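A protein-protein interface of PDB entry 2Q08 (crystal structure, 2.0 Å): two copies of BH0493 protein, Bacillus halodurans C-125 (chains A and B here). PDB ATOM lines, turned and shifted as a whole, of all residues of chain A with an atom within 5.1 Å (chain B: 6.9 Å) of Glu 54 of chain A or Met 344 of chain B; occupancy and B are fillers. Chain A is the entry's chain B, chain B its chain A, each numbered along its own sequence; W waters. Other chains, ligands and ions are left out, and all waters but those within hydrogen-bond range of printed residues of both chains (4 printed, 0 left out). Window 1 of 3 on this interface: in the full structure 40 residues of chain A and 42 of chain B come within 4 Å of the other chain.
Of the 16 printed residues of chain B, 10 touch a printed residue of chain A. Hydrophobic or aromatic side chains of chain B that line the printed part of chain A: His 307, Val 311, Ala 313, Met 344 and Leu 345. Hydrophobic or aromatic side chains of chain A within 4 Å of the printed part of chain B: Tyr 50, Ala 53, Trp 58 and Phe 327. Among the printed residues, 16 pairs touch across the chains. Among the printed residues, Asp or Glu carboxylates within 4 Å of a Lys or Arg side-chain nitrogen of the other chain: Glu 54 of chain A with Arg 314 of chain B (3.0 Å).
No position is printed for both chains.
The side-chain carboxylate of Glu 54 of chain A is in hydrogen-bond range of the side-chain sulfur of Cys 93 of chain A, at 3.8 Å. The guanidinium group of Arg 314 of chain B sits at hydrogen-bond distance from the backbone carbonyl oxygen of Met 344 of chain B (2.7 Å). The side-chain hydroxyl of Ser 90 of chain A sits at hydrogen-bond distance from the side-chain carboxylate of Glu 54 of chain A, at 2.7 Å. The backbone carbonyl oxygen (O) of Leu 345 of chain B sits at hydrogen-bond distance from the side-chain hydroxyl (OG) of Ser 348 of chain B. The backbone NH (N) of Cys 93 of chain A lies within hydrogen-bond range of the side-chain hydroxyl (OG) of Ser 90 of chain A (3.2 Å). O of Phe 327 of chain A sits at hydrogen-bond distance from ND2 of Asn 330 of chain A (3.0 Å).
Glu 54 of chain A touches two residues of chain B. Printed residues of chain A within 4 Å of Met 344 of chain B: Glu 54 (3.8 Å) and Asn 330 (3.4 Å). Printed residues of chain A within 4 Å of His 307 of chain B: Phe 327. Of the printed residues of chain B, Arg 57 of chain A touches Ala 313, Leu 345 and Ser 348. Of the printed residues of chain A, Val 311 of chain B touches Phe 327. Of the printed residues of chain A, Ser 348 of chain B touches Arg 57 and Trp 58. Cys 93 of chain A touches none of the printed residues of chain B. The nearest residue of chain B that does not touch Glu 54 of chain A is Glu 343 of chain B (4.8 Å). The nearest printed residue of chain A that does not touch Met 344 of chain B is Phe 327 of chain A (4.002 Å).
NH2 of Arg 314 of chain B lies within hydrogen-bond range of O of Tyr 50 of chain A. NH1 of Arg 57 of chain A is in hydrogen-bond range of O of Ala 313 of chain B. The backbone carbonyl oxygen (O) of Ser 348 of chain B sits at hydrogen-bond distance from the guanidinium group (NH2) of Arg 57 of chain A (2.8 Å). NH1 of Arg 314 of chain B is in salt-bridge range of OE2 of Glu 54 of chain A (3.0 Å). A ring nitrogen (NE2) of His 307 of chain B is in hydrogen-bond range of the backbone carbonyl oxygen of Phe 327 of chain A, at 2.9 Å.
Among the printed residues, pairs that only touch across the chains: Asn 330 of chain A with Glu 343 of chain B, Ala 53 of chain A with Arg 314 of chain B, Asn 330 of chain A with Met 344 of chain B, Ser 90 of chain A with Met 342 of chain B, Phe 327 of chain A with Val 311 of chain B, Arg 57 of chain A with Leu 345 of chain B, Trp 58 of chain A with Ser 348 of chain B, Ser 90 of chain A with Gly 346 of chain B, Ser 90 of chain A with Glu 343 of chain B, Glu 54 of chain A with Met 344 of chain B and Phe 327 of chain A with Arg 314 of chain B.
Water W4 lies within hydrogen-bond range of the side-chain carboxylate of Glu 54 of chain A (2.7 Å), the backbone carbonyl oxygen of Glu 343 of chain B (2.9 Å) and the backbone NH of Ala 92 of chain A (3.0 Å). Water W2 lies within hydrogen-bond range of OE1 of Glu 54 of chain A (2.7 Å) and O of Leu 345 of chain B (3.2 Å). Water W1 bridges O of Ala 53 of chain A (2.8 Å) and O of Arg 314 of chain B (2.8 Å). Water W3 lies within hydrogen-bond range of the side-chain hydroxyl of Ser 348 of chain B (2.9 Å), the backbone carbonyl oxygen of Glu 54 of chain A (2.9 Å) and the backbone carbonyl oxygen of Leu 345 of chain B (3.3 Å).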
ATOM      1  N   TYR A  50      20.960 -31.726 -20.962  1.00  0.00           N
ATOM      2  CA  TYR A  50      19.658 -31.394 -21.542  1.00  0.00           C
ATOM      3  C   TYR A  50      18.578 -31.803 -20.541  1.00  0.00           C
ATOM      4  O   TYR A  50      17.600 -31.082 -20.343  1.00  0.00           O
ATOM      5  CB  TYR A  50      19.418 -32.158 -22.851  1.00  0.00           C
ATOM      6  CG  TYR A  50      20.086 -31.597 -24.092  1.00  0.00           C
ATOM      7  CD1 TYR A  50      21.367 -31.050 -24.040  1.00  0.00           C
ATOM      8  CD2 TYR A  50      19.468 -31.709 -25.344  1.00  0.00           C
ATOM      9  CE1 TYR A  50      22.024 -30.635 -25.204  1.00  0.00           C
ATOM     10  CE2 TYR A  50      20.119 -31.299 -26.517  1.00  0.00           C
ATOM     11  CZ  TYR A  50      21.394 -30.767 -26.439  1.00  0.00           C
ATOM     12  OH  TYR A  50      22.047 -30.387 -27.586  1.00  0.00           O
ATOM     13  N   LEU A  51      18.763 -32.963 -19.911  1.00  0.00           N
ATOM     14  CA  LEU A  51      17.788 -33.468 -18.950  1.00  0.00           C
ATOM     15  C   LEU A  51      17.874 -32.783 -17.590  1.00  0.00           C
ATOM     16  O   LEU A  51      16.890 -32.741 -16.848  1.00  0.00           O
ATOM     17  CB  LEU A  51      17.930 -34.983 -18.809  1.00  0.00           C
ATOM     18  CG  LEU A  51      17.657 -35.747 -20.113  1.00  0.00           C
ATOM     19  CD1 LEU A  51      17.740 -37.251 -19.886  1.00  0.00           C
ATOM     20  CD2 LEU A  51      16.273 -35.368 -20.626  1.00  0.00           C
ATOM     21  N   VAL A  52      19.042 -32.244 -17.258  1.00  0.00           N
ATOM     22  CA  VAL A  52      19.195 -31.530 -15.994  1.00  0.00           C
ATOM     23  C   VAL A  52      18.295 -30.299 -16.070  1.00  0.00           C
ATOM     24  O   VAL A  52      17.515 -30.022 -15.154  1.00  0.00           O
ATOM     25  CB  VAL A  52      20.658 -31.088 -15.763  1.00  0.00           C
ATOM     26  CG1 VAL A  52      20.746 -30.175 -14.548  1.00  0.00           C
ATOM     27  CG2 VAL A  52      21.539 -32.320 -15.562  1.00  0.00           C
ATOM     28  N   ALA A  53      18.394 -29.573 -17.181  1.00  0.00           N
ATOM     29  CA  ALA A  53      17.562 -28.391 -17.385  1.00  0.00           C
ATOM     30  C   ALA A  53      16.089 -28.767 -17.244  1.00  0.00           C
ATOM     31  O   ALA A  53      15.339 -28.102 -16.540  1.00  0.00           O
ATOM     32  CB  ALA A  53      17.819 -27.796 -18.773  1.00  0.00           C
ATOM     33  N   GLU A  54      15.684 -29.841 -17.908  1.00  0.00           N
ATOM     34  CA  GLU A  54      14.291 -30.273 -17.867  1.00  0.00           C
ATOM     35  C   GLU A  54      13.793 -30.739 -16.498  1.00  0.00           C
ATOM     36  O   GLU A  54      12.672 -30.407 -16.098  1.00  0.00           O
ATOM     37  CB  GLU A  54      14.053 -31.366 -18.917  1.00  0.00           C
ATOM     38  CG  GLU A  54      14.050 -30.807 -20.348  1.00  0.00           C
ATOM     39  CD  GLU A  54      13.941 -31.880 -21.417  1.00  0.00           C
ATOM     40  OE1 GLU A  54      13.135 -32.813 -21.249  1.00  0.00           O
ATOM     41  OE2 GLU A  54      14.657 -31.769 -22.439  1.00  0.00           O
ATOM     42  N   VAL A  55      14.609 -31.497 -15.772  1.00  0.00           N
ATOM     43  CA  VAL A  55      14.168 -31.973 -14.459  1.00  0.00           C
ATOM     44  C   VAL A  55      14.015 -30.790 -13.491  1.00  0.00           C
ATOM     45  O   VAL A  55      13.104 -30.767 -12.651  1.00  0.00           O
ATOM     46  CB  VAL A  55      15.151 -33.022 -13.870  1.00  0.00           C
ATOM     47  CG1 VAL A  55      16.466 -32.356 -13.455  1.00  0.00           C
ATOM     48  CG2 VAL A  55      14.497 -33.745 -12.694  1.00  0.00           C
ATOM     49  N   MET A  56      14.881 -29.790 -13.628  1.00  0.00           N
ATOM     50  CA  MET A  56      14.797 -28.629 -12.751  1.00  0.00           C
ATOM     51  C   MET A  56      13.512 -27.822 -12.932  1.00  0.00           C
ATOM     52  O   MET A  56      13.159 -27.024 -12.061  1.00  0.00           O
ATOM     53  CB  MET A  56      16.010 -27.722 -12.936  1.00  0.00           C
ATOM     54  CG  MET A  56      17.323 -28.313 -12.436  1.00  0.00           C
ATOM     55  SD  MET A  56      17.237 -29.012 -10.748  1.00  0.00           S
ATOM     56  CE  MET A  56      16.765 -27.618  -9.835  1.00  0.00           C
ATOM     57  N   ARG A  57      12.809 -28.021 -14.047  1.00  0.00           N
ATOM     58  CA  ARG A  57      11.549 -27.306 -14.262  1.00  0.00           C
ATOM     59  C   ARG A  57      10.429 -27.970 -13.473  1.00  0.00           C
ATOM     60  O   ARG A  57       9.387 -27.358 -13.229  1.00  0.00           O
ATOM     61  CB  ARG A  57      11.152 -27.283 -15.753  1.00  0.00           C
ATOM     62  CG  ARG A  57      11.906 -26.266 -16.607  1.00  0.00           C
ATOM     63  CD  ARG A  57      11.241 -26.072 -17.974  1.00  0.00           C
ATOM     64  NE  ARG A  57       9.863 -25.595 -17.863  1.00  0.00           N
ATOM     65  CZ  ARG A  57       9.512 -24.392 -17.411  1.00  0.00           C
ATOM     66  NH1 ARG A  57      10.438 -23.527 -17.024  1.00  0.00           N
ATOM     67  NH2 ARG A  57       8.237 -24.054 -17.340  1.00  0.00           N
ATOM     68  N   TRP A  58      10.646 -29.220 -13.073  1.00  0.00           N
ATOM     69  CA  TRP A  58       9.635 -29.978 -12.342  1.00  0.00           C
ATOM     70  C   TRP A  58       9.911 -30.233 -10.859  1.00  0.00           C
ATOM     71  O   TRP A  58       9.052 -30.000 -10.014  1.00  0.00           O
ATOM     72  CB  TRP A  58       9.415 -31.344 -13.007  1.00  0.00           C
ATOM     73  CG  TRP A  58       8.540 -31.343 -14.218  1.00  0.00           C
ATOM     74  CD1 TRP A  58       8.900 -31.700 -15.491  1.00  0.00           C
ATOM     75  CD2 TRP A  58       7.139 -31.057 -14.264  1.00  0.00           C
ATOM     76  NE1 TRP A  58       7.809 -31.663 -16.318  1.00  0.00           N
ATOM     77  CE2 TRP A  58       6.713 -31.270 -15.596  1.00  0.00           C
ATOM     78  CE3 TRP A  58       6.199 -30.643 -13.311  1.00  0.00           C
ATOM     79  CZ2 TRP A  58       5.387 -31.085 -16.000  1.00  0.00           C
ATOM     80  CZ3 TRP A  58       4.873 -30.458 -13.712  1.00  0.00           C
ATOM     81  CH2 TRP A  58       4.482 -30.682 -15.049  1.00  0.00           C
ATOM     82  N   LEU A  82      10.911 -37.091 -14.887  1.00  0.00           N
ATOM     83  CA  LEU A  82      10.635 -36.921 -16.318  1.00  0.00           C
ATOM     84  C   LEU A  82      10.060 -38.110 -17.081  1.00  0.00           C
ATOM     85  O   LEU A  82       9.533 -37.934 -18.184  1.00  0.00           O
ATOM     86  CB  LEU A  82      11.901 -36.445 -17.036  1.00  0.00           C
ATOM     87  CG  LEU A  82      12.531 -35.145 -16.529  1.00  0.00           C
ATOM     88  CD1 LEU A  82      13.729 -34.799 -17.387  1.00  0.00           C
ATOM     89  CD2 LEU A  82      11.511 -34.020 -16.549  1.00  0.00           C
ATOM     90  N   SER A  90       9.404 -35.284 -24.317  1.00  0.00           N
ATOM     91  CA  SER A  90      10.365 -34.327 -24.870  1.00  0.00           C
ATOM     92  C   SER A  90      11.361 -35.077 -25.754  1.00  0.00           C
ATOM     93  O   SER A  90      11.515 -36.291 -25.634  1.00  0.00           O
ATOM     94  CB  SER A  90      11.118 -33.577 -23.764  1.00  0.00           C
ATOM     95  OG  SER A  90      12.122 -34.387 -23.168  1.00  0.00           O
ATOM     96  N   ALA A  92      14.678 -34.955 -25.783  1.00  0.00           N
ATOM     97  CA  ALA A  92      15.779 -35.529 -25.013  1.00  0.00           C
ATOM     98  C   ALA A  92      15.378 -36.799 -24.268  1.00  0.00           C
ATOM     99  O   ALA A  92      16.154 -37.745 -24.212  1.00  0.00           O
ATOM    100  CB  ALA A  92      16.335 -34.500 -24.032  1.00  0.00           C
ATOM    101  N   CYS A  93      14.176 -36.822 -23.690  1.00  0.00           N
ATOM    102  CA  CYS A  93      13.718 -38.012 -22.966  1.00  0.00           C
ATOM    103  C   CYS A  93      13.430 -39.138 -23.949  1.00  0.00           C
ATOM    104  O   CYS A  93      13.781 -40.289 -23.711  1.00  0.00           O
ATOM    105  CB  CYS A  93      12.471 -37.688 -22.142  1.00  0.00           C
ATOM    106  SG  CYS A  93      12.824 -36.566 -20.771  1.00  0.00           S
ATOM    107  N   PHE A 327      19.634 -26.339 -29.491  1.00  0.00           N
ATOM    108  CA  PHE A 327      18.230 -25.932 -29.450  1.00  0.00           C
ATOM    109  C   PHE A 327      17.544 -26.059 -30.813  1.00  0.00           C
ATOM    110  O   PHE A 327      16.321 -25.936 -30.907  1.00  0.00           O
ATOM    111  CB  PHE A 327      18.116 -24.510 -28.907  1.00  0.00           C
ATOM    112  CG  PHE A 327      18.799 -24.323 -27.576  1.00  0.00           C
ATOM    113  CD1 PHE A 327      18.498 -25.161 -26.496  1.00  0.00           C
ATOM    114  CD2 PHE A 327      19.762 -23.339 -27.407  1.00  0.00           C
ATOM    115  CE1 PHE A 327      19.160 -25.019 -25.266  1.00  0.00           C
ATOM    116  CE2 PHE A 327      20.431 -23.185 -26.178  1.00  0.00           C
ATOM    117  CZ  PHE A 327      20.122 -24.035 -25.108  1.00  0.00           C
ATOM    118  N   ASN A 330      15.678 -30.388 -32.695  1.00  0.00           N
ATOM    119  CA  ASN A 330      14.347 -30.842 -32.312  1.00  0.00           C
ATOM    120  C   ASN A 330      13.594 -31.067 -33.623  1.00  0.00           C
ATOM    121  O   ASN A 330      13.716 -30.265 -34.539  1.00  0.00           O
ATOM    122  CB  ASN A 330      13.685 -29.764 -31.447  1.00  0.00           C
ATOM    123  CG  ASN A 330      14.380 -29.597 -30.107  1.00  0.00           C
ATOM    124  OD1 ASN A 330      14.251 -30.447 -29.228  1.00  0.00           O
ATOM    125  ND2 ASN A 330      15.138 -28.516 -29.948  1.00  0.00           N
ATOM    126  N   GLN B 306       9.440 -16.568 -30.106  1.00  0.00           N
ATOM    127  CA  GLN B 306       8.955 -17.846 -29.597  1.00  0.00           C
ATOM    128  C   GLN B 306       9.956 -18.945 -29.288  1.00  0.00           C
ATOM    129  O   GLN B 306       9.902 -19.536 -28.209  1.00  0.00           O
ATOM    130  CB  GLN B 306       7.860 -18.395 -30.510  1.00  0.00           C
ATOM    131  CG  GLN B 306       6.669 -17.452 -30.715  1.00  0.00           C
ATOM    132  CD  GLN B 306       6.126 -16.878 -29.402  1.00  0.00           C
ATOM    133  OE1 GLN B 306       6.080 -17.560 -28.380  1.00  0.00           O
ATOM    134  NE2 GLN B 306       5.695 -15.623 -29.443  1.00  0.00           N
ATOM    135  N   HIS B 307      10.855 -19.238 -30.223  1.00  0.00           N
ATOM    136  CA  HIS B 307      11.832 -20.280 -29.977  1.00  0.00           C
ATOM    137  C   HIS B 307      12.783 -19.918 -28.825  1.00  0.00           C
ATOM    138  O   HIS B 307      13.014 -20.746 -27.943  1.00  0.00           O
ATOM    139  CB  HIS B 307      12.637 -20.585 -31.249  1.00  0.00           C
ATOM    140  CG  HIS B 307      13.741 -21.570 -31.029  1.00  0.00           C
ATOM    141  ND1 HIS B 307      14.985 -21.197 -30.571  1.00  0.00           N
ATOM    142  CD2 HIS B 307      13.760 -22.921 -31.108  1.00  0.00           C
ATOM    143  CE1 HIS B 307      15.721 -22.275 -30.370  1.00  0.00           C
ATOM    144  NE2 HIS B 307      15.000 -23.335 -30.687  1.00  0.00           N
ATOM    145  N   GLU B 308      13.331 -18.700 -28.823  1.00  0.00           N
ATOM    146  CA  GLU B 308      14.249 -18.311 -27.745  1.00  0.00           C
ATOM    147  C   GLU B 308      13.544 -18.234 -26.392  1.00  0.00           C
ATOM    148  O   GLU B 308      14.179 -18.418 -25.357  1.00  0.00           O
ATOM    149  CB  GLU B 308      14.970 -16.987 -28.065  1.00  0.00           C
ATOM    150  CG  GLU B 308      14.076 -15.810 -28.367  1.00  0.00           C
ATOM    151  CD  GLU B 308      14.827 -14.655 -28.996  1.00  0.00           C
ATOM    152  OE1 GLU B 308      15.994 -14.853 -29.400  1.00  0.00           O
ATOM    153  OE2 GLU B 308      14.247 -13.544 -29.098  1.00  0.00           O
ATOM    154  N   VAL B 310      11.251 -20.330 -25.475  1.00  0.00           N
ATOM    155  CA  VAL B 310      11.213 -21.724 -25.038  1.00  0.00           C
ATOM    156  C   VAL B 310      12.575 -22.074 -24.425  1.00  0.00           C
ATOM    157  O   VAL B 310      12.644 -22.712 -23.370  1.00  0.00           O
ATOM    158  CB  VAL B 310      10.935 -22.695 -26.208  1.00  0.00           C
ATOM    159  CG1 VAL B 310      10.995 -24.143 -25.702  1.00  0.00           C
ATOM    160  CG2 VAL B 310       9.565 -22.411 -26.826  1.00  0.00           C
ATOM    161  N   VAL B 311      13.656 -21.658 -25.084  1.00  0.00           N
ATOM    162  CA  VAL B 311      14.992 -21.943 -24.568  1.00  0.00           C
ATOM    163  C   VAL B 311      15.189 -21.271 -23.204  1.00  0.00           C
ATOM    164  O   VAL B 311      15.803 -21.846 -22.303  1.00  0.00           O
ATOM    165  CB  VAL B 311      16.092 -21.470 -25.546  1.00  0.00           C
ATOM    166  CG1 VAL B 311      17.484 -21.720 -24.941  1.00  0.00           C
ATOM    167  CG2 VAL B 311      15.974 -22.233 -26.872  1.00  0.00           C
ATOM    168  N   ALA B 313      12.991 -20.800 -20.986  1.00  0.00           N
ATOM    169  CA  ALA B 313      12.253 -21.614 -20.022  1.00  0.00           C
ATOM    170  C   ALA B 313      13.087 -22.829 -19.597  1.00  0.00           C
ATOM    171  O   ALA B 313      12.957 -23.308 -18.463  1.00  0.00           O
ATOM    172  CB  ALA B 313      10.928 -22.073 -20.617  1.00  0.00           C
ATOM    173  N   ARG B 314      13.921 -23.333 -20.508  1.00  0.00           N
ATOM    174  CA  ARG B 314      14.782 -24.467 -20.189  1.00  0.00           C
ATOM    175  C   ARG B 314      15.800 -24.031 -19.130  1.00  0.00           C
ATOM    176  O   ARG B 314      16.245 -24.845 -18.324  1.00  0.00           O
ATOM    177  CB  ARG B 314      15.559 -24.951 -21.423  1.00  0.00           C
ATOM    178  CG  ARG B 314      14.738 -25.686 -22.473  1.00  0.00           C
ATOM    179  CD  ARG B 314      15.635 -26.180 -23.611  1.00  0.00           C
ATOM    180  NE  ARG B 314      16.694 -27.073 -23.140  1.00  0.00           N
ATOM    181  CZ  ARG B 314      16.521 -28.355 -22.821  1.00  0.00           C
ATOM    182  NH1 ARG B 314      15.320 -28.915 -22.919  1.00  0.00           N
ATOM    183  NH2 ARG B 314      17.558 -29.091 -22.417  1.00  0.00           N
ATOM    184  N   ARG B 339       4.784 -27.462 -30.854  1.00  0.00           N
ATOM    185  CA  ARG B 339       5.749 -28.520 -31.109  1.00  0.00           C
ATOM    186  C   ARG B 339       7.130 -28.143 -30.556  1.00  0.00           C
ATOM    187  O   ARG B 339       7.797 -28.981 -29.952  1.00  0.00           O
ATOM    188  CB  ARG B 339       5.803 -28.823 -32.615  1.00  0.00           C
ATOM    189  CG  ARG B 339       4.562 -29.583 -33.084  1.00  0.00           C
ATOM    190  CD  ARG B 339       4.459 -29.733 -34.606  1.00  0.00           C
ATOM    191  NE  ARG B 339       3.228 -30.457 -34.941  1.00  0.00           N
ATOM    192  CZ  ARG B 339       3.100 -31.778 -34.853  1.00  0.00           C
ATOM    193  NH1 ARG B 339       4.131 -32.515 -34.460  1.00  0.00           N
ATOM    194  NH2 ARG B 339       1.941 -32.364 -35.128  1.00  0.00           N
ATOM    195  N   MET B 340       7.557 -26.892 -30.746  1.00  0.00           N
ATOM    196  CA  MET B 340       8.859 -26.455 -30.222  1.00  0.00           C
ATOM    197  C   MET B 340       8.856 -26.530 -28.693  1.00  0.00           C
ATOM    198  O   MET B 340       9.851 -26.929 -28.069  1.00  0.00           O
ATOM    199  CB  MET B 340       9.181 -25.005 -30.626  1.00  0.00           C
ATOM    200  CG  MET B 340       9.404 -24.790 -32.116  1.00  0.00           C
ATOM    201  SD  MET B 340      10.077 -23.178 -32.418  1.00  0.00           S
ATOM    202  CE  MET B 340       8.643 -22.073 -32.085  1.00  0.00           C
ATOM    203  N   ARG B 341       7.735 -26.136 -28.096  1.00  0.00           N
ATOM    204  CA  ARG B 341       7.606 -26.146 -26.644  1.00  0.00           C
ATOM    205  C   ARG B 341       7.664 -27.560 -26.065  1.00  0.00           C
ATOM    206  O   ARG B 341       8.412 -27.814 -25.123  1.00  0.00           O
ATOM    207  CB  ARG B 341       6.299 -25.456 -26.238  1.00  0.00           C
ATOM    208  CG  ARG B 341       6.347 -23.945 -26.422  1.00  0.00           C
ATOM    209  CD  ARG B 341       4.984 -23.315 -26.300  1.00  0.00           C
ATOM    210  NE  ARG B 341       5.083 -21.878 -26.101  1.00  0.00           N
ATOM    211  CZ  ARG B 341       4.046 -21.089 -25.833  1.00  0.00           C
ATOM    212  NH1 ARG B 341       2.829 -21.607 -25.737  1.00  0.00           N
ATOM    213  NH2 ARG B 341       4.231 -19.787 -25.632  1.00  0.00           N
ATOM    214  N   MET B 342       6.894 -28.486 -26.628  1.00  0.00           N
ATOM    215  CA  MET B 342       6.894 -29.848 -26.117  1.00  0.00           C
ATOM    216  C   MET B 342       8.234 -30.556 -26.368  1.00  0.00           C
ATOM    217  O   MET B 342       8.712 -31.335 -25.528  1.00  0.00           O
ATOM    218  CB  MET B 342       5.748 -30.654 -26.737  1.00  0.00           C
ATOM    219  CG  MET B 342       5.561 -32.020 -26.092  1.00  0.00           C
ATOM    220  SD  MET B 342       3.973 -32.775 -26.450  1.00  0.00           S
ATOM    221  CE  MET B 342       2.867 -31.615 -25.598  1.00  0.00           C
ATOM    222  N   GLU B 343       8.845 -30.288 -27.514  1.00  0.00           N
ATOM    223  CA  GLU B 343      10.127 -30.905 -27.828  1.00  0.00           C
ATOM    224  C   GLU B 343      11.231 -30.488 -26.849  1.00  0.00           C
ATOM    225  O   GLU B 343      12.091 -31.296 -26.495  1.00  0.00           O
ATOM    226  CB  GLU B 343      10.513 -30.590 -29.289  1.00  0.00           C
ATOM    227  CG  GLU B 343       9.769 -31.504 -30.267  1.00  0.00           C
ATOM    228  CD  GLU B 343       9.742 -31.047 -31.736  1.00  0.00           C
ATOM    229  OE1 GLU B 343      10.565 -30.199 -32.170  1.00  0.00           O
ATOM    230  OE2 GLU B 343       8.881 -31.584 -32.462  1.00  0.00           O
ATOM    231  N   MET B 344      11.194 -29.243 -26.378  1.00  0.00           N
ATOM    232  CA  MET B 344      12.219 -28.762 -25.451  1.00  0.00           C
ATOM    233  C   MET B 344      11.805 -28.685 -23.975  1.00  0.00           C
ATOM    234  O   MET B 344      12.662 -28.530 -23.105  1.00  0.00           O
ATOM    235  CB  MET B 344      12.734 -27.380 -25.891  1.00  0.00           C
ATOM    236  CG  MET B 344      13.785 -27.413 -26.992  1.00  0.00           C
ATOM    237  SD  MET B 344      14.327 -25.767 -27.441  1.00  0.00           S
ATOM    238  CE  MET B 344      12.975 -25.298 -28.573  1.00  0.00           C
ATOM    239  N   LEU B 345      10.509 -28.797 -23.692  1.00  0.00           N
ATOM    240  CA  LEU B 345      10.039 -28.696 -22.311  1.00  0.00           C
ATOM    241  C   LEU B 345       9.156 -29.852 -21.853  1.00  0.00           C
ATOM    242  O   LEU B 345       8.684 -29.853 -20.710  1.00  0.00           O
ATOM    243  CB  LEU B 345       9.256 -27.388 -22.122  1.00  0.00           C
ATOM    244  CG  LEU B 345       9.944 -26.078 -22.518  1.00  0.00           C
ATOM    245  CD1 LEU B 345       8.920 -24.943 -22.513  1.00  0.00           C
ATOM    246  CD2 LEU B 345      11.102 -25.784 -21.568  1.00  0.00           C
ATOM    247  N   GLY B 346       8.923 -30.828 -22.728  1.00  0.00           N
ATOM    248  CA  GLY B 346       8.059 -31.935 -22.357  1.00  0.00           C
ATOM    249  C   GLY B 346       6.668 -31.384 -22.075  1.00  0.00           C
ATOM    250  O   GLY B 346       6.063 -30.749 -22.941  1.00  0.00           O
ATOM    251  N   SER B 348       6.076 -29.387 -19.289  1.00  0.00           N
ATOM    252  CA  SER B 348       6.217 -28.287 -18.340  1.00  0.00           C
ATOM    253  C   SER B 348       5.929 -26.879 -18.873  1.00  0.00           C
ATOM    254  O   SER B 348       6.742 -25.981 -18.736  1.00  0.00           O
ATOM    255  CB  SER B 348       7.613 -28.326 -17.686  1.00  0.00           C
ATOM    256  OG  SER B 348       8.669 -28.102 -18.615  1.00  0.00           O
HETATM  257  O   HOH W   1      15.667 -25.499 -15.698  1.00  0.00           O
HETATM  258  O   HOH W   2      10.827 -32.189 -20.008  1.00  0.00           O
HETATM  259  O   HOH W   3      10.994 -29.817 -18.387  1.00  0.00           O
HETATM  260  O   HOH W   4      14.430 -32.098 -25.073  1.00  0.00           O
